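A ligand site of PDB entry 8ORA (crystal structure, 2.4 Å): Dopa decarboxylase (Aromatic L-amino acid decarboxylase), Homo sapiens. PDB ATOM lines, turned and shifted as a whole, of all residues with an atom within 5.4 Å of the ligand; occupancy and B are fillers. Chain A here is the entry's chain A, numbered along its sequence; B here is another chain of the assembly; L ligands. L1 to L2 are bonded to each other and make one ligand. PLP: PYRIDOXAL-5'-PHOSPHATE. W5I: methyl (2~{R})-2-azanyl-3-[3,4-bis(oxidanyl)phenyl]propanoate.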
ATOM      1  N   TRP A  71       2.944  11.526 -14.117  1.00  0.00           N
ATOM      2  CA  TRP A  71       2.665  10.117 -14.357  1.00  0.00           C
ATOM      3  C   TRP A  71       3.654   9.502 -15.325  1.00  0.00           C
ATOM      4  O   TRP A  71       3.865   8.286 -15.310  1.00  0.00           O
ATOM      5  CB  TRP A  71       1.233   9.941 -14.895  1.00  0.00           C
ATOM      6  CG  TRP A  71       0.178   9.934 -13.843  1.00  0.00           C
ATOM      7  CD1 TRP A  71      -0.163  10.968 -13.014  1.00  0.00           C
ATOM      8  CD2 TRP A  71      -0.702   8.852 -13.511  1.00  0.00           C
ATOM      9  NE1 TRP A  71      -1.200  10.587 -12.190  1.00  0.00           N
ATOM     10  CE2 TRP A  71      -1.547   9.288 -12.478  1.00  0.00           C
ATOM     11  CE3 TRP A  71      -0.844   7.544 -13.995  1.00  0.00           C
ATOM     12  CZ2 TRP A  71      -2.520   8.479 -11.914  1.00  0.00           C
ATOM     13  CZ3 TRP A  71      -1.819   6.739 -13.440  1.00  0.00           C
ATOM     14  CH2 TRP A  71      -2.641   7.205 -12.409  1.00  0.00           C
ATOM     15  N   TYR A  79       0.194   3.248  -8.810  1.00  0.00           N
ATOM     16  CA  TYR A  79      -1.045   2.765  -9.393  1.00  0.00           C
ATOM     17  C   TYR A  79      -0.798   1.834 -10.568  1.00  0.00           C
ATOM     18  O   TYR A  79      -0.228   0.756 -10.417  1.00  0.00           O
ATOM     19  CB  TYR A  79      -1.922   3.935  -9.836  1.00  0.00           C
ATOM     20  CG  TYR A  79      -2.000   5.083  -8.849  1.00  0.00           C
ATOM     21  CD1 TYR A  79      -2.703   4.960  -7.661  1.00  0.00           C
ATOM     22  CD2 TYR A  79      -1.361   6.288  -9.116  1.00  0.00           C
ATOM     23  CE1 TYR A  79      -2.779   6.005  -6.764  1.00  0.00           C
ATOM     24  CE2 TYR A  79      -1.427   7.337  -8.221  1.00  0.00           C
ATOM     25  CZ  TYR A  79      -2.138   7.197  -7.049  1.00  0.00           C
ATOM     26  OH  TYR A  79      -2.202   8.236  -6.158  1.00  0.00           O
ATOM     27  N   PHE A  80      -1.241   2.247 -11.749  1.00  0.00           N
ATOM     28  CA  PHE A  80      -1.030   1.552 -13.000  1.00  0.00           C
ATOM     29  C   PHE A  80      -0.641   2.582 -14.049  1.00  0.00           C
ATOM     30  O   PHE A  80      -0.932   3.770 -13.889  1.00  0.00           O
ATOM     31  CB  PHE A  80      -2.286   0.785 -13.438  1.00  0.00           C
ATOM     32  CG  PHE A  80      -2.360  -0.611 -12.891  1.00  0.00           C
ATOM     33  CD1 PHE A  80      -1.221  -1.396 -12.783  1.00  0.00           C
ATOM     34  CD2 PHE A  80      -3.576  -1.144 -12.474  1.00  0.00           C
ATOM     35  CE1 PHE A  80      -1.291  -2.679 -12.277  1.00  0.00           C
ATOM     36  CE2 PHE A  80      -3.645  -2.427 -11.968  1.00  0.00           C
ATOM     37  CZ  PHE A  80      -2.502  -3.197 -11.865  1.00  0.00           C
ATOM     38  N   PRO A  81       0.017   2.159 -15.135  1.00  0.00           N
ATOM     39  CA  PRO A  81       0.407   3.124 -16.168  1.00  0.00           C
ATOM     40  C   PRO A  81      -0.807   3.789 -16.805  1.00  0.00           C
ATOM     41  O   PRO A  81      -1.887   3.213 -16.873  1.00  0.00           O
ATOM     42  CB  PRO A  81       1.170   2.267 -17.181  1.00  0.00           C
ATOM     43  CG  PRO A  81       0.724   0.873 -16.918  1.00  0.00           C
ATOM     44  CD  PRO A  81       0.492   0.805 -15.443  1.00  0.00           C
ATOM     45  N   THR A  82      -0.601   5.015 -17.266  1.00  0.00           N
ATOM     46  CA  THR A  82      -1.558   5.704 -18.118  1.00  0.00           C
ATOM     47  C   THR A  82      -0.881   6.048 -19.437  1.00  0.00           C
ATOM     48  O   THR A  82       0.340   6.225 -19.489  1.00  0.00           O
ATOM     49  CB  THR A  82      -2.127   6.963 -17.440  1.00  0.00           C
ATOM     50  OG1 THR A  82      -3.317   7.391 -18.143  1.00  0.00           O
ATOM     51  CG2 THR A  82      -1.117   8.096 -17.443  1.00  0.00           C
ATOM     52  N   GLY A 146     -15.887   5.750 -21.799  1.00  0.00           N
ATOM     53  CA  GLY A 146     -15.062   6.753 -21.159  1.00  0.00           C
ATOM     54  C   GLY A 146     -14.142   6.181 -20.101  1.00  0.00           C
ATOM     55  O   GLY A 146     -13.065   6.719 -19.848  1.00  0.00           O
ATOM     56  N   SER A 147     -14.549   5.086 -19.457  1.00  0.00           N
ATOM     57  CA  SER A 147     -13.758   4.489 -18.393  1.00  0.00           C
ATOM     58  C   SER A 147     -14.184   3.044 -18.203  1.00  0.00           C
ATOM     59  O   SER A 147     -15.277   2.644 -18.626  1.00  0.00           O
ATOM     60  CB  SER A 147     -13.904   5.264 -17.087  1.00  0.00           C
ATOM     61  OG  SER A 147     -15.188   5.039 -16.517  1.00  0.00           O
ATOM     62  N   ALA A 148     -13.314   2.261 -17.574  1.00  0.00           N
ATOM     63  CA  ALA A 148     -13.677   0.902 -17.203  1.00  0.00           C
ATOM     64  C   ALA A 148     -14.761   0.891 -16.136  1.00  0.00           C
ATOM     65  O   ALA A 148     -15.576  -0.042 -16.088  1.00  0.00           O
ATOM     66  CB  ALA A 148     -12.446   0.134 -16.717  1.00  0.00           C
ATOM     67  N   SER A 149     -14.790   1.909 -15.274  1.00  0.00           N
ATOM     68  CA  SER A 149     -15.852   2.016 -14.270  1.00  0.00           C
ATOM     69  C   SER A 149     -17.202   2.223 -14.935  1.00  0.00           C
ATOM     70  O   SER A 149     -18.208   1.656 -14.502  1.00  0.00           O
ATOM     71  CB  SER A 149     -15.545   3.164 -13.314  1.00  0.00           C
ATOM     72  OG  SER A 149     -14.249   3.033 -12.760  1.00  0.00           O
ATOM     73  N   GLU A 150     -17.238   3.026 -16.000  1.00  0.00           N
ATOM     74  CA  GLU A 150     -18.488   3.220 -16.748  1.00  0.00           C
ATOM     75  C   GLU A 150     -18.884   1.949 -17.482  1.00  0.00           C
ATOM     76  O   GLU A 150     -20.078   1.615 -17.540  1.00  0.00           O
ATOM     77  CB  GLU A 150     -18.332   4.390 -17.716  1.00  0.00           C
ATOM     78  CG  GLU A 150     -18.318   5.755 -17.066  1.00  0.00           C
ATOM     79  CD  GLU A 150     -17.761   6.832 -17.965  1.00  0.00           C
ATOM     80  OE1 GLU A 150     -16.533   7.045 -17.946  1.00  0.00           O
ATOM     81  OE2 GLU A 150     -18.555   7.469 -18.698  1.00  0.00           O
ATOM     82  N   HIS A 192     -11.865  -4.010  -8.120  1.00  0.00           N
ATOM     83  CA  HIS A 192     -11.751  -2.563  -8.060  1.00  0.00           C
ATOM     84  C   HIS A 192     -13.000  -1.950  -7.426  1.00  0.00           C
ATOM     85  O   HIS A 192     -14.074  -2.556  -7.409  1.00  0.00           O
ATOM     86  CB  HIS A 192     -11.529  -1.985  -9.462  1.00  0.00           C
ATOM     87  CG  HIS A 192     -11.196  -0.524  -9.480  1.00  0.00           C
ATOM     88  ND1 HIS A 192     -12.146   0.458  -9.632  1.00  0.00           N
ATOM     89  CD2 HIS A 192     -10.008   0.121  -9.382  1.00  0.00           C
ATOM     90  CE1 HIS A 192     -11.569   1.642  -9.615  1.00  0.00           C
ATOM     91  NE2 HIS A 192     -10.264   1.463  -9.464  1.00  0.00           N
ATOM     92  N   SER A 194     -14.848   0.149  -8.544  1.00  0.00           N
ATOM     93  CA  SER A 194     -15.888   0.447  -9.528  1.00  0.00           C
ATOM     94  C   SER A 194     -17.038  -0.550  -9.455  1.00  0.00           C
ATOM     95  O   SER A 194     -18.182  -0.194  -9.787  1.00  0.00           O
ATOM     96  CB  SER A 194     -15.288   0.467 -10.929  1.00  0.00           C
ATOM     97  OG  SER A 194     -14.474  -0.667 -11.160  1.00  0.00           O
ATOM     98  N   THR A 242     -12.288 -10.348 -12.580  1.00  0.00           N
ATOM     99  CA  THR A 242     -11.209  -9.402 -12.794  1.00  0.00           C
ATOM    100  C   THR A 242      -9.955 -10.124 -13.276  1.00  0.00           C
ATOM    101  O   THR A 242      -9.512 -11.092 -12.656  1.00  0.00           O
ATOM    102  CB  THR A 242     -10.901  -8.611 -11.516  1.00  0.00           C
ATOM    103  OG1 THR A 242     -12.087  -7.924 -11.088  1.00  0.00           O
ATOM    104  CG2 THR A 242      -9.792  -7.604 -11.766  1.00  0.00           C
ATOM    105  N   LEU A 243      -9.384  -9.643 -14.376  1.00  0.00           N
ATOM    106  CA  LEU A 243      -8.098 -10.094 -14.879  1.00  0.00           C
ATOM    107  C   LEU A 243      -7.084  -8.972 -14.653  1.00  0.00           C
ATOM    108  O   LEU A 243      -7.253  -7.878 -15.178  1.00  0.00           O
ATOM    109  CB  LEU A 243      -8.172 -10.470 -16.360  1.00  0.00           C
ATOM    110  CG  LEU A 243      -9.119 -11.615 -16.734  1.00  0.00           C
ATOM    111  CD1 LEU A 243      -9.100 -11.856 -18.231  1.00  0.00           C
ATOM    112  CD2 LEU A 243      -8.739 -12.887 -15.978  1.00  0.00           C
ATOM    113  N   GLY A 244      -6.046  -9.259 -13.875  1.00  0.00           N
ATOM    114  CA  GLY A 244      -5.105  -8.232 -13.497  1.00  0.00           C
ATOM    115  C   GLY A 244      -5.686  -7.311 -12.452  1.00  0.00           C
ATOM    116  O   GLY A 244      -6.057  -6.169 -12.742  1.00  0.00           O
ATOM    117  N   THR A 245      -5.773  -7.794 -11.217  1.00  0.00           N
ATOM    118  CA  THR A 245      -6.387  -7.032 -10.146  1.00  0.00           C
ATOM    119  C   THR A 245      -5.569  -5.786  -9.809  1.00  0.00           C
ATOM    120  O   THR A 245      -4.344  -5.758  -9.973  1.00  0.00           O
ATOM    121  CB  THR A 245      -6.546  -7.896  -8.896  1.00  0.00           C
ATOM    122  OG1 THR A 245      -5.300  -8.521  -8.573  1.00  0.00           O
ATOM    123  CG2 THR A 245      -7.608  -8.963  -9.120  1.00  0.00           C
ATOM    124  N   THR A 246      -6.278  -4.754  -9.346  1.00  0.00           N
ATOM    125  CA  THR A 246      -5.614  -3.526  -8.915  1.00  0.00           C
ATOM    126  C   THR A 246      -4.623  -3.791  -7.793  1.00  0.00           C
ATOM    127  O   THR A 246      -3.548  -3.171  -7.749  1.00  0.00           O
ATOM    128  CB  THR A 246      -6.682  -2.523  -8.462  1.00  0.00           C
ATOM    129  OG1 THR A 246      -7.429  -2.062  -9.597  1.00  0.00           O
ATOM    130  CG2 THR A 246      -6.064  -1.334  -7.748  1.00  0.00           C
ATOM    131  N   ASP A 271     -13.438  -7.695 -16.269  1.00  0.00           N
ATOM    132  CA  ASP A 271     -12.719  -6.443 -16.086  1.00  0.00           C
ATOM    133  C   ASP A 271     -11.221  -6.742 -16.167  1.00  0.00           C
ATOM    134  O   ASP A 271     -10.649  -7.309 -15.230  1.00  0.00           O
ATOM    135  CB  ASP A 271     -13.086  -5.795 -14.753  1.00  0.00           C
ATOM    136  CG  ASP A 271     -12.404  -4.447 -14.531  1.00  0.00           C
ATOM    137  OD1 ASP A 271     -11.690  -3.963 -15.449  1.00  0.00           O
ATOM    138  OD2 ASP A 271     -12.585  -3.866 -13.449  1.00  0.00           O
ATOM    139  N   ALA A 273      -8.821  -4.192 -17.161  1.00  0.00           N
ATOM    140  CA  ALA A 273      -8.446  -2.844 -17.551  1.00  0.00           C
ATOM    141  C   ALA A 273      -6.956  -2.727 -17.847  1.00  0.00           C
ATOM    142  O   ALA A 273      -6.552  -2.193 -18.885  1.00  0.00           O
ATOM    143  CB  ALA A 273      -8.842  -1.856 -16.451  1.00  0.00           C
ATOM    144  N   TYR A 274      -6.111  -3.239 -16.947  1.00  0.00           N
ATOM    145  CA  TYR A 274      -4.672  -3.127 -17.122  1.00  0.00           C
ATOM    146  C   TYR A 274      -4.089  -4.289 -17.917  1.00  0.00           C
ATOM    147  O   TYR A 274      -3.317  -4.077 -18.858  1.00  0.00           O
ATOM    148  CB  TYR A 274      -3.974  -3.012 -15.764  1.00  0.00           C
ATOM    149  CG  TYR A 274      -2.489  -3.259 -15.819  1.00  0.00           C
ATOM    150  CD1 TYR A 274      -1.632  -2.360 -16.439  1.00  0.00           C
ATOM    151  CD2 TYR A 274      -1.933  -4.408 -15.261  1.00  0.00           C
ATOM    152  CE1 TYR A 274      -0.278  -2.591 -16.502  1.00  0.00           C
ATOM    153  CE2 TYR A 274      -0.577  -4.643 -15.314  1.00  0.00           C
ATOM    154  CZ  TYR A 274       0.254  -3.729 -15.933  1.00  0.00           C
ATOM    155  OH  TYR A 274       1.608  -3.959 -15.995  1.00  0.00           O
ATOM    156  N   ASN A 300      -8.696  -1.311 -20.724  1.00  0.00           N
ATOM    157  CA  ASN A 300      -8.418   0.103 -20.928  1.00  0.00           C
ATOM    158  C   ASN A 300      -7.189   0.281 -21.798  1.00  0.00           C
ATOM    159  O   ASN A 300      -6.057   0.081 -21.327  1.00  0.00           O
ATOM    160  CB  ASN A 300      -8.214   0.808 -19.577  1.00  0.00           C
ATOM    161  CG  ASN A 300      -9.515   1.004 -18.826  1.00  0.00           C
ATOM    162  OD1 ASN A 300     -10.601   0.951 -19.409  1.00  0.00           O
ATOM    163  ND2 ASN A 300      -9.411   1.261 -17.527  1.00  0.00           N
ATOM    164  N   HIS A 302      -6.194   3.128 -22.498  1.00  0.00           N
ATOM    165  CA  HIS A 302      -5.595   4.314 -21.904  1.00  0.00           C
ATOM    166  C   HIS A 302      -4.734   3.982 -20.693  1.00  0.00           C
ATOM    167  O   HIS A 302      -4.305   4.894 -19.982  1.00  0.00           O
ATOM    168  CB  HIS A 302      -6.671   5.347 -21.536  1.00  0.00           C
ATOM    169  CG  HIS A 302      -7.662   4.878 -20.515  1.00  0.00           C
ATOM    170  ND1 HIS A 302      -9.021   5.058 -20.675  1.00  0.00           N
ATOM    171  CD2 HIS A 302      -7.504   4.263 -19.327  1.00  0.00           C
ATOM    172  CE1 HIS A 302      -9.658   4.566 -19.633  1.00  0.00           C
ATOM    173  NE2 HIS A 302      -8.759   4.065 -18.796  1.00  0.00           N
ATOM    174  N   LYS A 303      -4.471   2.700 -20.452  1.00  0.00           N
ATOM    175  CA  LYS A 303      -3.523   2.262 -19.442  1.00  0.00           C
ATOM    176  C   LYS A 303      -2.226   1.771 -20.066  1.00  0.00           C
ATOM    177  O   LYS A 303      -1.172   2.372 -19.857  1.00  0.00           O
ATOM    178  CB  LYS A 303      -4.137   1.148 -18.592  1.00  0.00           C
ATOM    179  CG  LYS A 303      -4.953   1.603 -17.422  1.00  0.00           C
ATOM    180  CD  LYS A 303      -5.497   0.388 -16.722  1.00  0.00           C
ATOM    181  CE  LYS A 303      -5.636   0.634 -15.251  1.00  0.00           C
ATOM    182  NZ  LYS A 303      -6.472   1.841 -15.017  1.00  0.00           N
ATOM    183  N   PHE A 309      -5.863   8.765 -22.510  1.00  0.00           N
ATOM    184  CA  PHE A 309      -7.176   8.924 -21.897  1.00  0.00           C
ATOM    185  C   PHE A 309      -7.937  10.058 -22.572  1.00  0.00           C
ATOM    186  O   PHE A 309      -7.372  11.133 -22.825  1.00  0.00           O
ATOM    187  CB  PHE A 309      -7.006   9.199 -20.393  1.00  0.00           C
ATOM    188  CG  PHE A 309      -8.275   9.130 -19.600  1.00  0.00           C
ATOM    189  CD1 PHE A 309      -9.030  10.272 -19.379  1.00  0.00           C
ATOM    190  CD2 PHE A 309      -8.716   7.935 -19.071  1.00  0.00           C
ATOM    191  CE1 PHE A 309     -10.204  10.217 -18.635  1.00  0.00           C
ATOM    192  CE2 PHE A 309      -9.887   7.872 -18.332  1.00  0.00           C
ATOM    193  CZ  PHE A 309     -10.630   9.009 -18.116  1.00  0.00           C
ATOM    194  N   ARG A 447       3.517  -1.768  -3.613  1.00  0.00           N
ATOM    195  CA  ARG A 447       3.366  -2.110  -5.017  1.00  0.00           C
ATOM    196  C   ARG A 447       4.396  -1.366  -5.857  1.00  0.00           C
ATOM    197  O   ARG A 447       4.672  -0.187  -5.596  1.00  0.00           O
ATOM    198  CB  ARG A 447       1.961  -1.778  -5.524  1.00  0.00           C
ATOM    199  CG  ARG A 447       0.835  -2.261  -4.635  1.00  0.00           C
ATOM    200  CD  ARG A 447      -0.489  -1.600  -5.002  1.00  0.00           C
ATOM    201  NE  ARG A 447      -0.971  -2.000  -6.323  1.00  0.00           N
ATOM    202  CZ  ARG A 447      -0.813  -1.298  -7.432  1.00  0.00           C
ATOM    203  NH1 ARG A 447      -0.168  -0.135  -7.429  1.00  0.00           N
ATOM    204  NH2 ARG A 447      -1.302  -1.764  -8.580  1.00  0.00           N
ATOM    205  N   ILE B 101      -4.197  11.586 -14.376  1.00  0.00           N
ATOM    206  CA  ILE B 101      -5.483  10.961 -14.106  1.00  0.00           C
ATOM    207  C   ILE B 101      -5.920  11.373 -12.706  1.00  0.00           C
ATOM    208  O   ILE B 101      -5.720  10.619 -11.746  1.00  0.00           O
ATOM    209  CB  ILE B 101      -5.425   9.435 -14.263  1.00  0.00           C
ATOM    210  CG1 ILE B 101      -4.730   9.059 -15.582  1.00  0.00           C
ATOM    211  CG2 ILE B 101      -6.820   8.831 -14.205  1.00  0.00           C
ATOM    212  CD1 ILE B 101      -5.419   9.616 -16.810  1.00  0.00           C
ATOM    213  N   PHE B 103      -8.011  11.326 -10.276  1.00  0.00           N
ATOM    214  CA  PHE B 103      -9.075  10.800  -9.431  1.00  0.00           C
ATOM    215  C   PHE B 103      -8.969  11.330  -8.012  1.00  0.00           C
ATOM    216  O   PHE B 103      -9.982  11.487  -7.332  1.00  0.00           O
ATOM    217  CB  PHE B 103      -9.056   9.273  -9.445  1.00  0.00           C
ATOM    218  CG  PHE B 103      -7.671   8.679  -9.453  1.00  0.00           C
ATOM    219  CD1 PHE B 103      -6.873   8.705  -8.324  1.00  0.00           C
ATOM    220  CD2 PHE B 103      -7.175   8.076 -10.605  1.00  0.00           C
ATOM    221  CE1 PHE B 103      -5.607   8.154  -8.342  1.00  0.00           C
ATOM    222  CE2 PHE B 103      -5.911   7.529 -10.631  1.00  0.00           C
ATOM    223  CZ  PHE B 103      -5.125   7.561  -9.498  1.00  0.00           C
ATOM    224  N   TYR B 332      -5.416   1.811  -2.100  1.00  0.00           N
ATOM    225  CA  TYR B 332      -4.635   2.206  -3.264  1.00  0.00           C
ATOM    226  C   TYR B 332      -5.044   3.568  -3.805  1.00  0.00           C
ATOM    227  O   TYR B 332      -4.324   4.125  -4.637  1.00  0.00           O
ATOM    228  CB  TYR B 332      -4.741   1.146  -4.360  1.00  0.00           C
ATOM    229  CG  TYR B 332      -6.145   0.667  -4.670  1.00  0.00           C
ATOM    230  CD1 TYR B 332      -6.974   1.386  -5.515  1.00  0.00           C
ATOM    231  CD2 TYR B 332      -6.637  -0.524  -4.128  1.00  0.00           C
ATOM    232  CE1 TYR B 332      -8.255   0.953  -5.809  1.00  0.00           C
ATOM    233  CE2 TYR B 332      -7.916  -0.960  -4.413  1.00  0.00           C
ATOM    234  CZ  TYR B 332      -8.721  -0.221  -5.265  1.00  0.00           C
ATOM    235  OH  TYR B 332      -9.990  -0.654  -5.551  1.00  0.00           O
ATOM    236  N   LEU B 333      -6.165   4.121  -3.350  1.00  0.00           N
ATOM    237  CA  LEU B 333      -6.607   5.465  -3.736  1.00  0.00           C
ATOM    238  C   LEU B 333      -6.634   6.406  -2.539  1.00  0.00           C
ATOM    239  O   LEU B 333      -7.383   7.394  -2.533  1.00  0.00           O
ATOM    240  CB  LEU B 333      -7.969   5.393  -4.421  1.00  0.00           C
ATOM    241  CG  LEU B 333      -7.933   4.686  -5.784  1.00  0.00           C
ATOM    242  CD1 LEU B 333      -9.311   4.456  -6.368  1.00  0.00           C
ATOM    243  CD2 LEU B 333      -7.063   5.474  -6.747  1.00  0.00           C
ATOM    244  N   PRO B 352     -17.519   8.112 -13.403  1.00  0.00           N
ATOM    245  CA  PRO B 352     -16.208   7.475 -13.547  1.00  0.00           C
ATOM    246  C   PRO B 352     -15.327   7.771 -12.340  1.00  0.00           C
ATOM    247  O   PRO B 352     -15.640   8.585 -11.471  1.00  0.00           O
ATOM    248  CB  PRO B 352     -15.642   8.098 -14.817  1.00  0.00           C
ATOM    249  CG  PRO B 352     -16.273   9.444 -14.868  1.00  0.00           C
ATOM    250  CD  PRO B 352     -17.665   9.242 -14.353  1.00  0.00           C
ATOM    251  N   LEU B 353     -14.184   7.084 -12.312  1.00  0.00           N
ATOM    252  CA  LEU B 353     -13.131   7.364 -11.352  1.00  0.00           C
ATOM    253  C   LEU B 353     -12.050   8.257 -11.937  1.00  0.00           C
ATOM    254  O   LEU B 353     -11.651   9.243 -11.320  1.00  0.00           O
ATOM    255  CB  LEU B 353     -12.501   6.055 -10.848  1.00  0.00           C
ATOM    256  CG  LEU B 353     -11.334   6.239  -9.868  1.00  0.00           C
ATOM    257  CD1 LEU B 353     -11.852   6.304  -8.436  1.00  0.00           C
ATOM    258  CD2 LEU B 353     -10.292   5.137 -10.024  1.00  0.00           C
ATOM    259  N   GLY B 354     -11.566   7.926 -13.132  1.00  0.00           N
ATOM    260  CA  GLY B 354     -10.554   8.718 -13.780  1.00  0.00           C
ATOM    261  C   GLY B 354     -11.109   9.979 -14.423  1.00  0.00           C
ATOM    262  O   GLY B 354     -12.291  10.081 -14.747  1.00  0.00           O
HETATM  263  N1  PLP L   1     -10.598  -1.846 -13.143  1.00  0.00           N
HETATM  264  C2  PLP L   1      -9.365  -2.156 -12.722  1.00  0.00           C
HETATM  265  C2A PLP L   1      -8.982  -3.493 -12.610  1.00  0.00           C
HETATM  266  C3  PLP L   1      -8.469  -1.135 -12.402  1.00  0.00           C
HETATM  267  O3  PLP L   1      -7.220  -1.463 -11.982  1.00  0.00           O
HETATM  268  C4  PLP L   1      -8.810   0.205 -12.500  1.00  0.00           C
HETATM  269  C4A PLP L   1      -7.863   1.200 -12.170  1.00  0.00           C
HETATM  270  C5  PLP L   1     -10.089   0.525 -12.940  1.00  0.00           C
HETATM  271  C6  PLP L   1     -10.982  -0.506 -13.264  1.00  0.00           C
HETATM  272  C5A PLP L   1     -10.491   1.851 -13.064  1.00  0.00           C
HETATM  273  O4P PLP L   1     -10.900   2.103 -14.412  1.00  0.00           O
HETATM  274  P   PLP L   1     -10.965   3.607 -14.969  1.00  0.00           P
HETATM  275  O1P PLP L   1     -12.446   4.054 -14.557  1.00  0.00           O
HETATM  276  O2P PLP L   1     -10.880   3.541 -16.437  1.00  0.00           O
HETATM  277  O3P PLP L   1      -9.980   4.430 -14.210  1.00  0.00           O
HETATM  278  N1  W5I L   2      -6.448   1.414 -12.149  1.00  0.00           N
HETATM  279  C2  W5I L   2      -5.840   4.192 -12.726  1.00  0.00           C
HETATM  280  C3  W5I L   2      -6.935   4.784 -13.343  1.00  0.00           C
HETATM  281  C4  W5I L   2      -6.806   5.167 -14.678  1.00  0.00           C
HETATM  282  C5  W5I L   2      -5.613   4.967 -15.361  1.00  0.00           C
HETATM  283  C6  W5I L   2      -4.519   4.383 -14.739  1.00  0.00           C
HETATM  284  C7  W5I L   2      -5.889   3.786 -11.398  1.00  0.00           C
HETATM  285  C8  W5I L   2      -6.713   2.515 -11.185  1.00  0.00           C
HETATM  286  C9  W5I L   2      -6.591   2.153  -9.675  1.00  0.00           C
HETATM  287  C10 W5I L   2      -4.416   0.965  -9.768  1.00  0.00           C
HETATM  288  C1  W5I L   2      -4.648   3.995 -13.418  1.00  0.00           C
HETATM  289  O1  W5I L   2      -5.573   5.379 -16.662  1.00  0.00           O
HETATM  290  O2  W5I L   2      -7.815   5.763 -15.369  1.00  0.00           O
HETATM  291  O3  W5I L   2      -7.269   3.114  -8.870  1.00  0.00           O
HETATM  292  O4  W5I L   2      -5.228   1.991  -9.183  1.00  0.00           O
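The side-chain hydroxyl of Thr 82 is in hydrogen-bond range of an oxygen (O1) of W5I L2, at 3.4 Å. O1P of PLP L1 sits at hydrogen-bond distance from OG of Ser 149 (2.7 Å). NZ of Lys 303 lies close to N1 of W5I L2, at 2.9 Å. OG1 of Thr 246 sits at hydrogen-bond distance from O3 of PLP L1, 2.5 Å away. A ring nitrogen (NE2) of His 192 sits at hydrogen-bond distance from an oxygen (O3) of W5I L2. O2P of PLP L1 lies within hydrogen-bond range of NE2 of His 302, at 3.2 Å. The side-chain amide nitrogen (ND2) of Asn 300 lies within hydrogen-bond range of an oxygen (O2P) of PLP L1 (2.9 Å). The backbone NH (N) of Ala 148 sits at hydrogen-bond distance from an oxygen (O2P) of PLP L1 (3.0 Å). OD2 of Asp 271 sits at hydrogen-bond distance from N1 of PLP L1, 2.8 Å away. N of Ser 149 lies within hydrogen-bond range of O1P of PLP L1 (3.3 Å).
OD1 of Asp 271 is in hydrogen-bond range of N of Ala 273 (3.3 Å). The backbone carbonyl oxygen (O) of His 302 sits at hydrogen-bond distance from the side-chain hydroxyl (OG1) of Thr 82. The side-chain amide nitrogen (ND2) of Asn 300 sits at hydrogen-bond distance from a ring nitrogen (NE2) of His 302 (3.1 Å). NH2 of Arg 447 is in hydrogen-bond range of O of Thr 246 (2.8 Å). The backbone carbonyl oxygen (O) of Tyr 79 sits at hydrogen-bond distance from the guanidinium group (NH1) of Arg 447 (3.1 Å). O of Ala 273 lies within hydrogen-bond range of N of Asn 300, 3.0 Å away. N of Leu 243 lies within hydrogen-bond range of O of Asp 271 (2.8 Å). The side-chain hydroxyl (OG) of Ser 147 lies within hydrogen-bond range of the side-chain carboxylate (OE1) of Glu 150 (2.8 Å).
Merely in contact with the ligand: Trp 71 (3.8 Å), Tyr 79 (3.8 Å), Phe 80 (3.5 Å), Pro 81 (3.6 Å), Ser 147 (3.2 Å), Gly 244 (3.97 Å), Ala 273 (3.7 Å), Ile 101 of chain B (3.4 Å), Phe 103 of chain B (3.8 Å), Tyr 332 of chain B (3.8 Å), Leu 333 of chain B (3.2 Å), Leu 353 of chain B (3.8 Å) and Gly 354 of chain B (3.99 Å). Hydrophobic or aromatic side chains within 4 Å of the ligand: Trp 71, Tyr 79, Phe 80, Ala 148, His 192, Ala 273, His 302, Ile 101 of chain B, Phe 103 of chain B, Tyr 332 of chain B, Leu 333 of chain B and Leu 353 of chain B. Of the 32 residues printed, 22 come within 4 Å of the ligand.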
